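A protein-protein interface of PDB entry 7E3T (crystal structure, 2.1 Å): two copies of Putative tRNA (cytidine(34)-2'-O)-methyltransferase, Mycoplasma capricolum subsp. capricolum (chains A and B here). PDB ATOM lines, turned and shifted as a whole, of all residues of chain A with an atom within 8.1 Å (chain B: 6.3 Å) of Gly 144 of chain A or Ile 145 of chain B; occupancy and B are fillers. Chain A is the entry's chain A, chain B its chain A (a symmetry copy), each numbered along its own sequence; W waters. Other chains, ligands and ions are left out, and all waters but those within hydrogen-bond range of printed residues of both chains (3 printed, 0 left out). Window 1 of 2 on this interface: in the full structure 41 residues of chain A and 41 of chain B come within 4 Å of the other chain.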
ATOM      1  N   ILE A   8      14.957   2.247  35.537  1.00  0.00           N
ATOM      2  CA  ILE A   8      13.622   1.611  35.407  1.00  0.00           C
ATOM      3  C   ILE A   8      13.733   0.226  36.002  1.00  0.00           C
ATOM      4  O   ILE A   8      14.664  -0.494  35.598  1.00  0.00           O
ATOM      5  CB  ILE A   8      13.227   1.560  33.925  1.00  0.00           C
ATOM      6  CG1 ILE A   8      13.253   2.970  33.337  1.00  0.00           C
ATOM      7  CG2 ILE A   8      11.880   0.876  33.738  1.00  0.00           C
ATOM      8  CD1 ILE A   8      12.326   3.945  34.056  1.00  0.00           C
ATOM      9  N   ALA A  21       9.332  -3.006  24.280  1.00  0.00           N
ATOM     10  CA  ALA A  21       8.985  -1.586  24.101  1.00  0.00           C
ATOM     11  C   ALA A  21       9.705  -0.737  25.138  1.00  0.00           C
ATOM     12  O   ALA A  21      10.191   0.347  24.789  1.00  0.00           O
ATOM     13  CB  ALA A  21       7.487  -1.395  24.167  1.00  0.00           C
ATOM     14  N   ILE A  22       9.798  -1.223  26.374  1.00  0.00           N
ATOM     15  CA  ILE A  22      10.499  -0.495  27.458  1.00  0.00           C
ATOM     16  C   ILE A  22      11.992  -0.400  27.110  1.00  0.00           C
ATOM     17  O   ILE A  22      12.605   0.669  27.352  1.00  0.00           O
ATOM     18  CB  ILE A  22      10.233  -1.187  28.796  1.00  0.00           C
ATOM     19  CG1 ILE A  22       8.750  -1.009  29.171  1.00  0.00           C
ATOM     20  CG2 ILE A  22      11.157  -0.655  29.877  1.00  0.00           C
ATOM     21  CD1 ILE A  22       8.280  -1.833  30.341  1.00  0.00           C
ATOM     22  N   THR A  25      12.536   2.453  24.844  1.00  0.00           N
ATOM     23  CA  THR A  25      12.448   3.733  25.577  1.00  0.00           C
ATOM     24  C   THR A  25      13.748   3.980  26.333  1.00  0.00           C
ATOM     25  O   THR A  25      14.260   5.100  26.234  1.00  0.00           O
ATOM     26  CB  THR A  25      11.212   3.791  26.488  1.00  0.00           C
ATOM     27  OG1 THR A  25      10.091   3.779  25.599  1.00  0.00           O
ATOM     28  CG2 THR A  25      11.199   5.051  27.317  1.00  0.00           C
ATOM     29  N   CYS A  26      14.250   2.971  27.045  1.00  0.00           N
ATOM     30  CA  CYS A  26      15.483   3.039  27.867  1.00  0.00           C
ATOM     31  C   CYS A  26      16.696   3.447  27.020  1.00  0.00           C
ATOM     32  O   CYS A  26      17.484   4.272  27.475  1.00  0.00           O
ATOM     33  CB  CYS A  26      15.744   1.704  28.531  1.00  0.00           C
ATOM     34  SG  CYS A  26      14.643   1.422  29.946  1.00  0.00           S
ATOM     35  N   ILE A  29      16.509   7.276  25.976  1.00  0.00           N
ATOM     36  CA  ILE A  29      16.776   8.291  27.035  1.00  0.00           C
ATOM     37  C   ILE A  29      18.017   7.894  27.836  1.00  0.00           C
ATOM     38  O   ILE A  29      18.220   8.494  28.870  1.00  0.00           O
ATOM     39  CB  ILE A  29      15.546   8.495  27.939  1.00  0.00           C
ATOM     40  CG1 ILE A  29      15.252   7.302  28.851  1.00  0.00           C
ATOM     41  CG2 ILE A  29      14.349   8.855  27.088  1.00  0.00           C
ATOM     42  CD1 ILE A  29      14.217   7.602  29.920  1.00  0.00           C
ATOM     43  N   LEU A 104      12.503   4.248  39.256  1.00  0.00           N
ATOM     44  CA  LEU A 104      11.034   4.161  38.977  1.00  0.00           C
ATOM     45  C   LEU A 104      10.668   2.685  38.873  1.00  0.00           C
ATOM     46  O   LEU A 104      11.283   1.982  38.061  1.00  0.00           O
ATOM     47  CB  LEU A 104      10.681   4.941  37.708  1.00  0.00           C
ATOM     48  CG  LEU A 104      11.131   6.399  37.678  1.00  0.00           C
ATOM     49  CD1 LEU A 104      10.836   7.068  36.363  1.00  0.00           C
ATOM     50  CD2 LEU A 104      10.509   7.192  38.810  1.00  0.00           C
ATOM     51  N   PHE A 106       7.975  -0.482  38.324  1.00  0.00           N
ATOM     52  CA  PHE A 106       6.730  -0.843  37.600  1.00  0.00           C
ATOM     53  C   PHE A 106       6.489  -2.347  37.797  1.00  0.00           C
ATOM     54  O   PHE A 106       7.439  -3.139  37.696  1.00  0.00           O
ATOM     55  CB  PHE A 106       6.832  -0.452  36.118  1.00  0.00           C
ATOM     56  CG  PHE A 106       7.176   0.982  35.853  1.00  0.00           C
ATOM     57  CD1 PHE A 106       8.483   1.436  35.923  1.00  0.00           C
ATOM     58  CD2 PHE A 106       6.187   1.896  35.534  1.00  0.00           C
ATOM     59  CE1 PHE A 106       8.791   2.773  35.709  1.00  0.00           C
ATOM     60  CE2 PHE A 106       6.497   3.223  35.279  1.00  0.00           C
ATOM     61  CZ  PHE A 106       7.799   3.669  35.381  1.00  0.00           C
ATOM     62  N   ILE A 128      -0.643   7.501  37.727  1.00  0.00           N
ATOM     63  CA  ILE A 128      -0.856   8.229  36.448  1.00  0.00           C
ATOM     64  C   ILE A 128      -2.339   8.562  36.450  1.00  0.00           C
ATOM     65  O   ILE A 128      -3.154   7.642  36.402  1.00  0.00           O
ATOM     66  CB  ILE A 128      -0.475   7.363  35.221  1.00  0.00           C
ATOM     67  CG1 ILE A 128       0.849   6.610  35.411  1.00  0.00           C
ATOM     68  CG2 ILE A 128      -0.485   8.190  33.941  1.00  0.00           C
ATOM     69  CD1 ILE A 128       2.077   7.402  35.092  1.00  0.00           C
ATOM     70  N   ASN A 138      -1.220   0.756  28.924  1.00  0.00           N
ATOM     71  CA  ASN A 138      -0.132  -0.223  28.733  1.00  0.00           C
ATOM     72  C   ASN A 138       1.051   0.188  29.627  1.00  0.00           C
ATOM     73  O   ASN A 138       1.391   1.373  29.686  1.00  0.00           O
ATOM     74  CB  ASN A 138       0.254  -0.317  27.258  1.00  0.00           C
ATOM     75  CG  ASN A 138       1.527  -1.107  27.125  1.00  0.00           C
ATOM     76  OD1 ASN A 138       2.597  -0.508  27.154  1.00  0.00           O
ATOM     77  ND2 ASN A 138       1.419  -2.432  27.138  1.00  0.00           N
ATOM     78  N   ILE A 139       1.663  -0.780  30.292  1.00  0.00           N
ATOM     79  CA  ILE A 139       2.836  -0.598  31.191  1.00  0.00           C
ATOM     80  C   ILE A 139       3.986   0.138  30.471  1.00  0.00           C
ATOM     81  O   ILE A 139       4.590   1.031  31.086  1.00  0.00           O
ATOM     82  CB  ILE A 139       3.231  -1.970  31.785  1.00  0.00           C
ATOM     83  CG1 ILE A 139       4.026  -1.805  33.079  1.00  0.00           C
ATOM     84  CG2 ILE A 139       3.944  -2.866  30.789  1.00  0.00           C
ATOM     85  CD1 ILE A 139       3.131  -1.436  34.278  1.00  0.00           C
ATOM     86  N   ALA A 140       4.293  -0.190  29.224  1.00  0.00           N
ATOM     87  CA  ALA A 140       5.374   0.463  28.431  1.00  0.00           C
ATOM     88  C   ALA A 140       5.095   1.965  28.308  1.00  0.00           C
ATOM     89  O   ALA A 140       6.026   2.774  28.452  1.00  0.00           O
ATOM     90  CB  ALA A 140       5.506  -0.147  27.064  1.00  0.00           C
ATOM     91  N   ASN A 141       3.836   2.338  28.067  1.00  0.00           N
ATOM     92  CA  ASN A 141       3.464   3.770  27.922  1.00  0.00           C
ATOM     93  C   ASN A 141       3.648   4.470  29.273  1.00  0.00           C
ATOM     94  O   ASN A 141       4.086   5.636  29.260  1.00  0.00           O
ATOM     95  CB  ASN A 141       2.080   3.931  27.296  1.00  0.00           C
ATOM     96  CG  ASN A 141       1.796   5.363  26.886  1.00  0.00           C
ATOM     97  OD1 ASN A 141       2.692   6.233  26.859  1.00  0.00           O
ATOM     98  ND2 ASN A 141       0.531   5.618  26.579  1.00  0.00           N
ATOM     99  N   THR A 142       3.367   3.783  30.396  1.00  0.00           N
ATOM    100  CA  THR A 142       3.528   4.357  31.758  1.00  0.00           C
ATOM    101  C   THR A 142       5.016   4.627  32.019  1.00  0.00           C
ATOM    102  O   THR A 142       5.315   5.632  32.682  1.00  0.00           O
ATOM    103  CB  THR A 142       2.893   3.509  32.879  1.00  0.00           C
ATOM    104  OG1 THR A 142       3.488   2.223  32.975  1.00  0.00           O
ATOM    105  CG2 THR A 142       1.393   3.374  32.700  1.00  0.00           C
ATOM    106  N   VAL A 143       5.918   3.727  31.612  1.00  0.00           N
ATOM    107  CA  VAL A 143       7.393   3.945  31.786  1.00  0.00           C
ATOM    108  C   VAL A 143       7.789   5.248  31.074  1.00  0.00           C
ATOM    109  O   VAL A 143       8.495   6.114  31.688  1.00  0.00           O
ATOM    110  CB  VAL A 143       8.187   2.727  31.296  1.00  0.00           C
ATOM    111  CG1 VAL A 143       9.678   3.015  31.255  1.00  0.00           C
ATOM    112  CG2 VAL A 143       7.874   1.531  32.160  1.00  0.00           C
ATOM    113  N   GLY A 144       7.249   5.488  29.884  1.00  0.00           N
ATOM    114  CA  GLY A 144       7.559   6.717  29.130  1.00  0.00           C
ATOM    115  C   GLY A 144       7.047   7.977  29.830  1.00  0.00           C
ATOM    116  O   GLY A 144       7.781   9.013  29.914  1.00  0.00           O
ATOM    117  N   ILE A 145       5.789   7.954  30.254  1.00  0.00           N
ATOM    118  CA  ILE A 145       5.142   9.130  30.888  1.00  0.00           C
ATOM    119  C   ILE A 145       5.903   9.455  32.176  1.00  0.00           C
ATOM    120  O   ILE A 145       6.223  10.614  32.436  1.00  0.00           O
ATOM    121  CB  ILE A 145       3.658   8.810  31.152  1.00  0.00           C
ATOM    122  CG1 ILE A 145       2.879   8.649  29.853  1.00  0.00           C
ATOM    123  CG2 ILE A 145       3.058   9.864  32.057  1.00  0.00           C
ATOM    124  CD1 ILE A 145       1.688   7.722  30.001  1.00  0.00           C
ATOM    125  N   ALA A 146       6.210   8.461  32.975  1.00  0.00           N
ATOM    126  CA  ALA A 146       6.893   8.705  34.265  1.00  0.00           C
ATOM    127  C   ALA A 146       8.341   9.183  34.028  1.00  0.00           C
ATOM    128  O   ALA A 146       8.784  10.192  34.679  1.00  0.00           O
ATOM    129  CB  ALA A 146       6.830   7.463  35.082  1.00  0.00           C
ATOM    130  N   SER A 147       9.073   8.509  33.136  1.00  0.00           N
ATOM    131  CA  SER A 147      10.468   8.873  32.790  1.00  0.00           C
ATOM    132  C   SER A 147      10.528  10.326  32.337  1.00  0.00           C
ATOM    133  O   SER A 147      11.441  11.026  32.774  1.00  0.00           O
ATOM    134  CB  SER A 147      11.012   7.972  31.742  1.00  0.00           C
ATOM    135  OG  SER A 147      11.127   6.681  32.286  1.00  0.00           O
ATOM    136  N   TYR A 148       9.660  10.741  31.425  1.00  0.00           N
ATOM    137  CA  TYR A 148       9.777  12.078  30.789  1.00  0.00           C
ATOM    138  C   TYR A 148       9.340  13.179  31.767  1.00  0.00           C
ATOM    139  O   TYR A 148       9.797  14.319  31.548  1.00  0.00           O
ATOM    140  CB  TYR A 148       9.092  12.122  29.428  1.00  0.00           C
ATOM    141  CG  TYR A 148       9.985  11.685  28.298  1.00  0.00           C
ATOM    142  CD1 TYR A 148      10.824  12.598  27.672  1.00  0.00           C
ATOM    143  CD2 TYR A 148      10.002  10.365  27.850  1.00  0.00           C
ATOM    144  CE1 TYR A 148      11.688  12.216  26.644  1.00  0.00           C
ATOM    145  CE2 TYR A 148      10.840   9.972  26.812  1.00  0.00           C
ATOM    146  CZ  TYR A 148      11.724  10.890  26.247  1.00  0.00           C
ATOM    147  OH  TYR A 148      12.495  10.524  25.209  1.00  0.00           O
ATOM    148  N   GLU A 149       8.569  12.857  32.818  1.00  0.00           N
ATOM    149  CA  GLU A 149       8.239  13.837  33.896  1.00  0.00           C
ATOM    150  C   GLU A 149       9.507  14.130  34.720  1.00  0.00           C
ATOM    151  O   GLU A 149       9.825  15.327  34.912  1.00  0.00           O
ATOM    152  CB  GLU A 149       7.088  13.383  34.801  1.00  0.00           C
ATOM    153  CG  GLU A 149       6.780  14.361  35.946  1.00  0.00           C
ATOM    154  CD  GLU A 149       6.772  15.867  35.674  1.00  0.00           C
ATOM    155  OE1 GLU A 149       6.537  16.290  34.523  1.00  0.00           O
ATOM    156  OE2 GLU A 149       7.018  16.643  36.639  1.00  0.00           O
ATOM    157  N   VAL A 150      10.234  13.099  35.142  1.00  0.00           N
ATOM    158  CA  VAL A 150      11.547  13.269  35.833  1.00  0.00           C
ATOM    159  C   VAL A 150      12.498  14.037  34.908  1.00  0.00           C
ATOM    160  O   VAL A 150      13.158  15.002  35.395  1.00  0.00           O
ATOM    161  CB  VAL A 150      12.155  11.938  36.302  1.00  0.00           C
ATOM    162  CG1 VAL A 150      13.472  12.174  37.037  1.00  0.00           C
ATOM    163  CG2 VAL A 150      11.204  11.153  37.203  1.00  0.00           C
ATOM    164  N   LEU A 151      12.554  13.668  33.622  1.00  0.00           N
ATOM    165  CA  LEU A 151      13.486  14.296  32.651  1.00  0.00           C
ATOM    166  C   LEU A 151      13.150  15.785  32.470  1.00  0.00           C
ATOM    167  O   LEU A 151      14.100  16.608  32.384  1.00  0.00           O
ATOM    168  CB  LEU A 151      13.474  13.546  31.320  1.00  0.00           C
ATOM    169  CG  LEU A 151      14.214  12.209  31.319  1.00  0.00           C
ATOM    170  CD1 LEU A 151      13.984  11.500  30.013  1.00  0.00           C
ATOM    171  CD2 LEU A 151      15.711  12.377  31.559  1.00  0.00           C
ATOM    172  N   TYR A 156      15.967  17.747  30.915  1.00  0.00           N
ATOM    173  CA  TYR A 156      16.183  16.714  29.862  1.00  0.00           C
ATOM    174  C   TYR A 156      17.672  16.364  29.757  1.00  0.00           C
ATOM    175  O   TYR A 156      18.053  15.800  28.719  1.00  0.00           O
ATOM    176  CB  TYR A 156      15.612  17.181  28.521  1.00  0.00           C
ATOM    177  CG  TYR A 156      14.118  17.367  28.511  1.00  0.00           C
ATOM    178  CD1 TYR A 156      13.252  16.276  28.493  1.00  0.00           C
ATOM    179  CD2 TYR A 156      13.568  18.635  28.557  1.00  0.00           C
ATOM    180  CE1 TYR A 156      11.873  16.437  28.518  1.00  0.00           C
ATOM    181  CE2 TYR A 156      12.194  18.819  28.561  1.00  0.00           C
ATOM    182  CZ  TYR A 156      11.344  17.718  28.537  1.00  0.00           C
ATOM    183  OH  TYR A 156       9.996  17.931  28.552  1.00  0.00           O
ATOM    184  N   ILE B  90       7.681  19.718  23.968  1.00  0.00           N
ATOM    185  CA  ILE B  90       6.269  20.156  24.141  1.00  0.00           C
ATOM    186  C   ILE B  90       6.107  20.884  25.481  1.00  0.00           C
ATOM    187  O   ILE B  90       5.309  21.827  25.525  1.00  0.00           O
ATOM    188  CB  ILE B  90       5.266  18.996  23.973  1.00  0.00           C
ATOM    189  CG1 ILE B  90       3.843  19.529  24.092  1.00  0.00           C
ATOM    190  CG2 ILE B  90       5.515  17.873  24.963  1.00  0.00           C
ATOM    191  CD1 ILE B  90       2.923  19.044  23.027  1.00  0.00           C
ATOM    192  N   ILE B 128      10.211  15.141  20.999  1.00  0.00           N
ATOM    193  CA  ILE B 128      10.423  14.405  22.274  1.00  0.00           C
ATOM    194  C   ILE B 128      11.932  14.256  22.373  1.00  0.00           C
ATOM    195  O   ILE B 128      12.517  13.569  21.538  1.00  0.00           O
ATOM    196  CB  ILE B 128       9.720  13.024  22.266  1.00  0.00           C
ATOM    197  CG1 ILE B 128       8.296  13.083  21.694  1.00  0.00           C
ATOM    198  CG2 ILE B 128       9.756  12.381  23.647  1.00  0.00           C
ATOM    199  CD1 ILE B 128       7.240  13.489  22.672  1.00  0.00           C
ATOM    200  N   LEU B 137      11.111   6.406  19.506  1.00  0.00           N
ATOM    201  CA  LEU B 137      10.096   5.829  20.419  1.00  0.00           C
ATOM    202  C   LEU B 137       8.951   5.246  19.584  1.00  0.00           C
ATOM    203  O   LEU B 137       8.657   5.753  18.512  1.00  0.00           O
ATOM    204  CB  LEU B 137       9.605   6.944  21.349  1.00  0.00           C
ATOM    205  CG  LEU B 137      10.640   7.514  22.307  1.00  0.00           C
ATOM    206  CD1 LEU B 137      10.047   8.665  23.089  1.00  0.00           C
ATOM    207  CD2 LEU B 137      11.171   6.460  23.273  1.00  0.00           C
ATOM    208  N   ALA B 140       2.750   5.204  19.813  1.00  0.00           N
ATOM    209  CA  ALA B 140       1.750   5.114  20.915  1.00  0.00           C
ATOM    210  C   ALA B 140       2.331   5.720  22.197  1.00  0.00           C
ATOM    211  O   ALA B 140       1.621   6.455  22.901  1.00  0.00           O
ATOM    212  CB  ALA B 140       1.327   3.693  21.166  1.00  0.00           C
ATOM    213  N   ASN B 141       3.603   5.439  22.488  1.00  0.00           N
ATOM    214  CA  ASN B 141       4.256   5.971  23.712  1.00  0.00           C
ATOM    215  C   ASN B 141       4.391   7.492  23.582  1.00  0.00           C
ATOM    216  O   ASN B 141       4.217   8.172  24.611  1.00  0.00           O
ATOM    217  CB  ASN B 141       5.557   5.233  24.022  1.00  0.00           C
ATOM    218  CG  ASN B 141       6.094   5.564  25.401  1.00  0.00           C
ATOM    219  OD1 ASN B 141       5.411   6.181  26.245  1.00  0.00           O
ATOM    220  ND2 ASN B 141       7.339   5.166  25.629  1.00  0.00           N
ATOM    221  N   THR B 142       4.648   8.013  22.368  1.00  0.00           N
ATOM    222  CA  THR B 142       4.778   9.473  22.125  1.00  0.00           C
ATOM    223  C   THR B 142       3.425  10.151  22.385  1.00  0.00           C
ATOM    224  O   THR B 142       3.432  11.281  22.895  1.00  0.00           O
ATOM    225  CB  THR B 142       5.343   9.833  20.736  1.00  0.00           C
ATOM    226  OG1 THR B 142       4.499   9.383  19.685  1.00  0.00           O
ATOM    227  CG2 THR B 142       6.746   9.290  20.542  1.00  0.00           C
ATOM    228  N   VAL B 143       2.308   9.547  21.965  1.00  0.00           N
ATOM    229  CA  VAL B 143       0.946  10.122  22.227  1.00  0.00           C
ATOM    230  C   VAL B 143       0.761  10.283  23.744  1.00  0.00           C
ATOM    231  O   VAL B 143       0.337  11.391  24.215  1.00  0.00           O
ATOM    232  CB  VAL B 143      -0.145   9.264  21.576  1.00  0.00           C
ATOM    233  CG1 VAL B 143      -1.532   9.699  22.015  1.00  0.00           C
ATOM    234  CG2 VAL B 143       0.002   9.301  20.075  1.00  0.00           C
ATOM    235  N   GLY B 144       1.194   9.301  24.525  1.00  0.00           N
ATOM    236  CA  GLY B 144       1.070   9.371  25.993  1.00  0.00           C
ATOM    237  C   GLY B 144       1.922  10.486  26.600  1.00  0.00           C
ATOM    238  O   GLY B 144       1.446  11.245  27.502  1.00  0.00           O
ATOM    239  N   ILE B 145       3.187  10.554  26.201  1.00  0.00           N
ATOM    240  CA  ILE B 145       4.144  11.544  26.757  1.00  0.00           C
ATOM    241  C   ILE B 145       3.630  12.945  26.418  1.00  0.00           C
ATOM    242  O   ILE B 145       3.602  13.825  27.278  1.00  0.00           O
ATOM    243  CB  ILE B 145       5.544  11.278  26.170  1.00  0.00           C
ATOM    244  CG1 ILE B 145       6.110   9.947  26.650  1.00  0.00           C
ATOM    245  CG2 ILE B 145       6.462  12.440  26.484  1.00  0.00           C
ATOM    246  CD1 ILE B 145       7.080   9.338  25.657  1.00  0.00           C
ATOM    247  N   ALA B 146       3.213  13.167  25.194  1.00  0.00           N
ATOM    248  CA  ALA B 146       2.758  14.513  24.777  1.00  0.00           C
ATOM    249  C   ALA B 146       1.430  14.873  25.476  1.00  0.00           C
ATOM    250  O   ALA B 146       1.296  16.027  26.014  1.00  0.00           O
ATOM    251  CB  ALA B 146       2.646  14.541  23.294  1.00  0.00           C
ATOM    252  N   SER B 147       0.469  13.946  25.487  1.00  0.00           N
ATOM    253  CA  SER B 147      -0.846  14.146  26.144  1.00  0.00           C
ATOM    254  C   SER B 147      -0.643  14.527  27.605  1.00  0.00           C
ATOM    255  O   SER B 147      -1.325  15.446  28.058  1.00  0.00           O
ATOM    256  CB  SER B 147      -1.693  12.932  26.029  1.00  0.00           C
ATOM    257  OG  SER B 147      -2.020  12.748  24.674  1.00  0.00           O
ATOM    258  N   TYR B 148       0.179  13.793  28.342  1.00  0.00           N
ATOM    259  CA  TYR B 148       0.279  13.975  29.812  1.00  0.00           C
ATOM    260  C   TYR B 148       1.058  15.257  30.145  1.00  0.00           C
ATOM    261  O   TYR B 148       0.836  15.758  31.265  1.00  0.00           O
ATOM    262  CB  TYR B 148       0.791  12.718  30.506  1.00  0.00           C
ATOM    263  CG  TYR B 148      -0.304  11.748  30.864  1.00  0.00           C
ATOM    264  CD1 TYR B 148      -0.994  11.877  32.062  1.00  0.00           C
ATOM    265  CD2 TYR B 148      -0.659  10.704  30.011  1.00  0.00           C
ATOM    266  CE1 TYR B 148      -2.036  11.014  32.406  1.00  0.00           C
ATOM    267  CE2 TYR B 148      -1.680   9.821  30.349  1.00  0.00           C
ATOM    268  CZ  TYR B 148      -2.405  10.013  31.524  1.00  0.00           C
ATOM    269  OH  TYR B 148      -3.355   9.130  31.875  1.00  0.00           O
ATOM    270  N   GLU B 149       1.860  15.799  29.214  1.00  0.00           N
ATOM    271  CA  GLU B 149       2.521  17.125  29.404  1.00  0.00           C
ATOM    272  C   GLU B 149       1.454  18.235  29.350  1.00  0.00           C
ATOM    273  O   GLU B 149       1.428  19.076  30.279  1.00  0.00           O
ATOM    274  CB  GLU B 149       3.645  17.396  28.399  1.00  0.00           C
ATOM    275  CG  GLU B 149       4.292  18.782  28.552  1.00  0.00           C
ATOM    276  CD  GLU B 149       4.593  19.324  29.950  1.00  0.00           C
ATOM    277  OE1 GLU B 149       4.776  18.534  30.900  1.00  0.00           O
ATOM    278  OE2 GLU B 149       4.638  20.577  30.101  1.00  0.00           O
ATOM    279  N   VAL B 150       0.576  18.215  28.351  1.00  0.00           N
ATOM    280  CA  VAL B 150      -0.577  19.161  28.273  1.00  0.00           C
ATOM    281  C   VAL B 150      -1.443  18.991  29.527  1.00  0.00           C
ATOM    282  O   VAL B 150      -1.815  20.033  30.143  1.00  0.00           O
ATOM    283  CB  VAL B 150      -1.399  19.001  26.985  1.00  0.00           C
ATOM    284  CG1 VAL B 150      -2.536  20.017  26.938  1.00  0.00           C
ATOM    285  CG2 VAL B 150      -0.540  19.142  25.730  1.00  0.00           C
HETATM  286  O   HOH W   1      -0.773   5.377  23.699  1.00  0.00           O
HETATM  287  O   HOH W   2       8.207   2.366  26.837  1.00  0.00           O
HETATM  288  O   HOH W   3       8.992   3.533  23.021  1.00  0.00           O
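Water W2 lies within hydrogen-bond range of the side-chain hydroxyl (OG1) of Thr 25 of chain A (2.7 Å), the backbone carbonyl oxygen (O) of Ala 140 of chain A (2.7 Å), the side-chain amide nitrogen (ND2) of Asn 141 of chain B (3.2 Å) and the backbone carbonyl oxygen (O) of Ala 21 of chain A (3.5 Å).
Water W1 lies within hydrogen-bond range of the backbone carbonyl oxygen of Ala 140 of chain B and the side-chain amide nitrogen of Asn 141 of chain A.
Water W3 lies within hydrogen-bond range of the side-chain hydroxyl (OG1) of Thr 25 of chain A (2.8 Å) and the side-chain amide nitrogen (ND2) of Asn 141 of chain B (3.5 Å).
Of the printed residues of chain B, Ile 128 of chain A touches Tyr 148.
Printed residues of chain B within 4 Å of Ala 140 of chain A: Asn 141 (3.9 Å).
Gly 144 of chain A touches two residues of chain B.
Printed residues of chain B within 4 Å of Ile 145 of chain A: Gly 144 and Tyr 148.
Of the printed residues of chain B, Tyr 148 of chain A touches Ile 128, Leu 137 and Ile 145.
Thr 142 of chain B touches none of the printed residues of chain A.
Of chain A, only Asn 141 and Ile 145 come within 4 Å of Gly 144 of chain B.
No residue of chain A comes within 4 Å of Ala 146 of chain B.
Ile 128 of chain A touches Tyr 148 of chain B, and with the chains exchanged Tyr 148 of chain A touches Ile 128 of chain B.
Ala 140 of chain A touches Asn 141 of chain B, and with the chains exchanged Asn 141 of chain A touches Ala 140 of chain B.
Asn 141 of chain A touches its own counterpart, Asn 141 of chain B.
Asn 141 of chain A touches Gly 144 of chain B, and with the chains exchanged Gly 144 of chain A touches Asn 141 of chain B.
Of the 14 pairs that touch across the chains among the printed residues, 11 have their exchanged pair printed and touching as well.
The side-chain hydroxyl (OG1) of Thr 25 of chain A lies within hydrogen-bond range of the side-chain amide nitrogen (ND2) of Asn 141 of chain B.
OD1 of Asn 141 of chain A lies close to OD1 of Asn 141 of chain B.
Of the 14 printed residues of chain B, 7 touch a printed residue of chain A.
Along chain B the printed residues that touch a printed residue of chain A span positions 128 to 148.
Hydrophobic or aromatic side chains of chain A that line the printed part of chain B: Ile 128, Ile 145 and Tyr 148.
Among the printed residues, 14 pairs touch across the chains.
Among the printed residues, no Asp or Glu carboxylate lies within 4 Å of a Lys or Arg side-chain nitrogen of the other chain.
Among the printed residues, merely in contact across the chains: Ile 128 of chain A with Tyr 148 of chain B, Tyr 148 of chain A with Ile 128 of chain B, Gly 144 of chain A with Asn 141 of chain B, Asn 141 of chain A with Gly 144 of chain B, Thr 25 of chain A with Leu 137 of chain B, Tyr 148 of chain A with Leu 137 of chain B, Gly 144 of chain A with Ile 145 of chain B, Ile 145 of chain A with Gly 144 of chain B, Ile 145 of chain A with Tyr 148 of chain B, Tyr 148 of chain A with Ile 145 of chain B, Ala 140 of chain A with Asn 141 of chain B and Asn 141 of chain A with Ala 140 of chain B.
The side-chain amide oxygen (OD1) of Asn 138 of chain A sits at hydrogen-bond distance from the backbone NH (N) of Ala 140 of chain A, at 2.7 Å.
The backbone NH (N) of Asn 141 of chain A lies within hydrogen-bond range of the side-chain amide oxygen (OD1) of Asn 138 of chain A.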
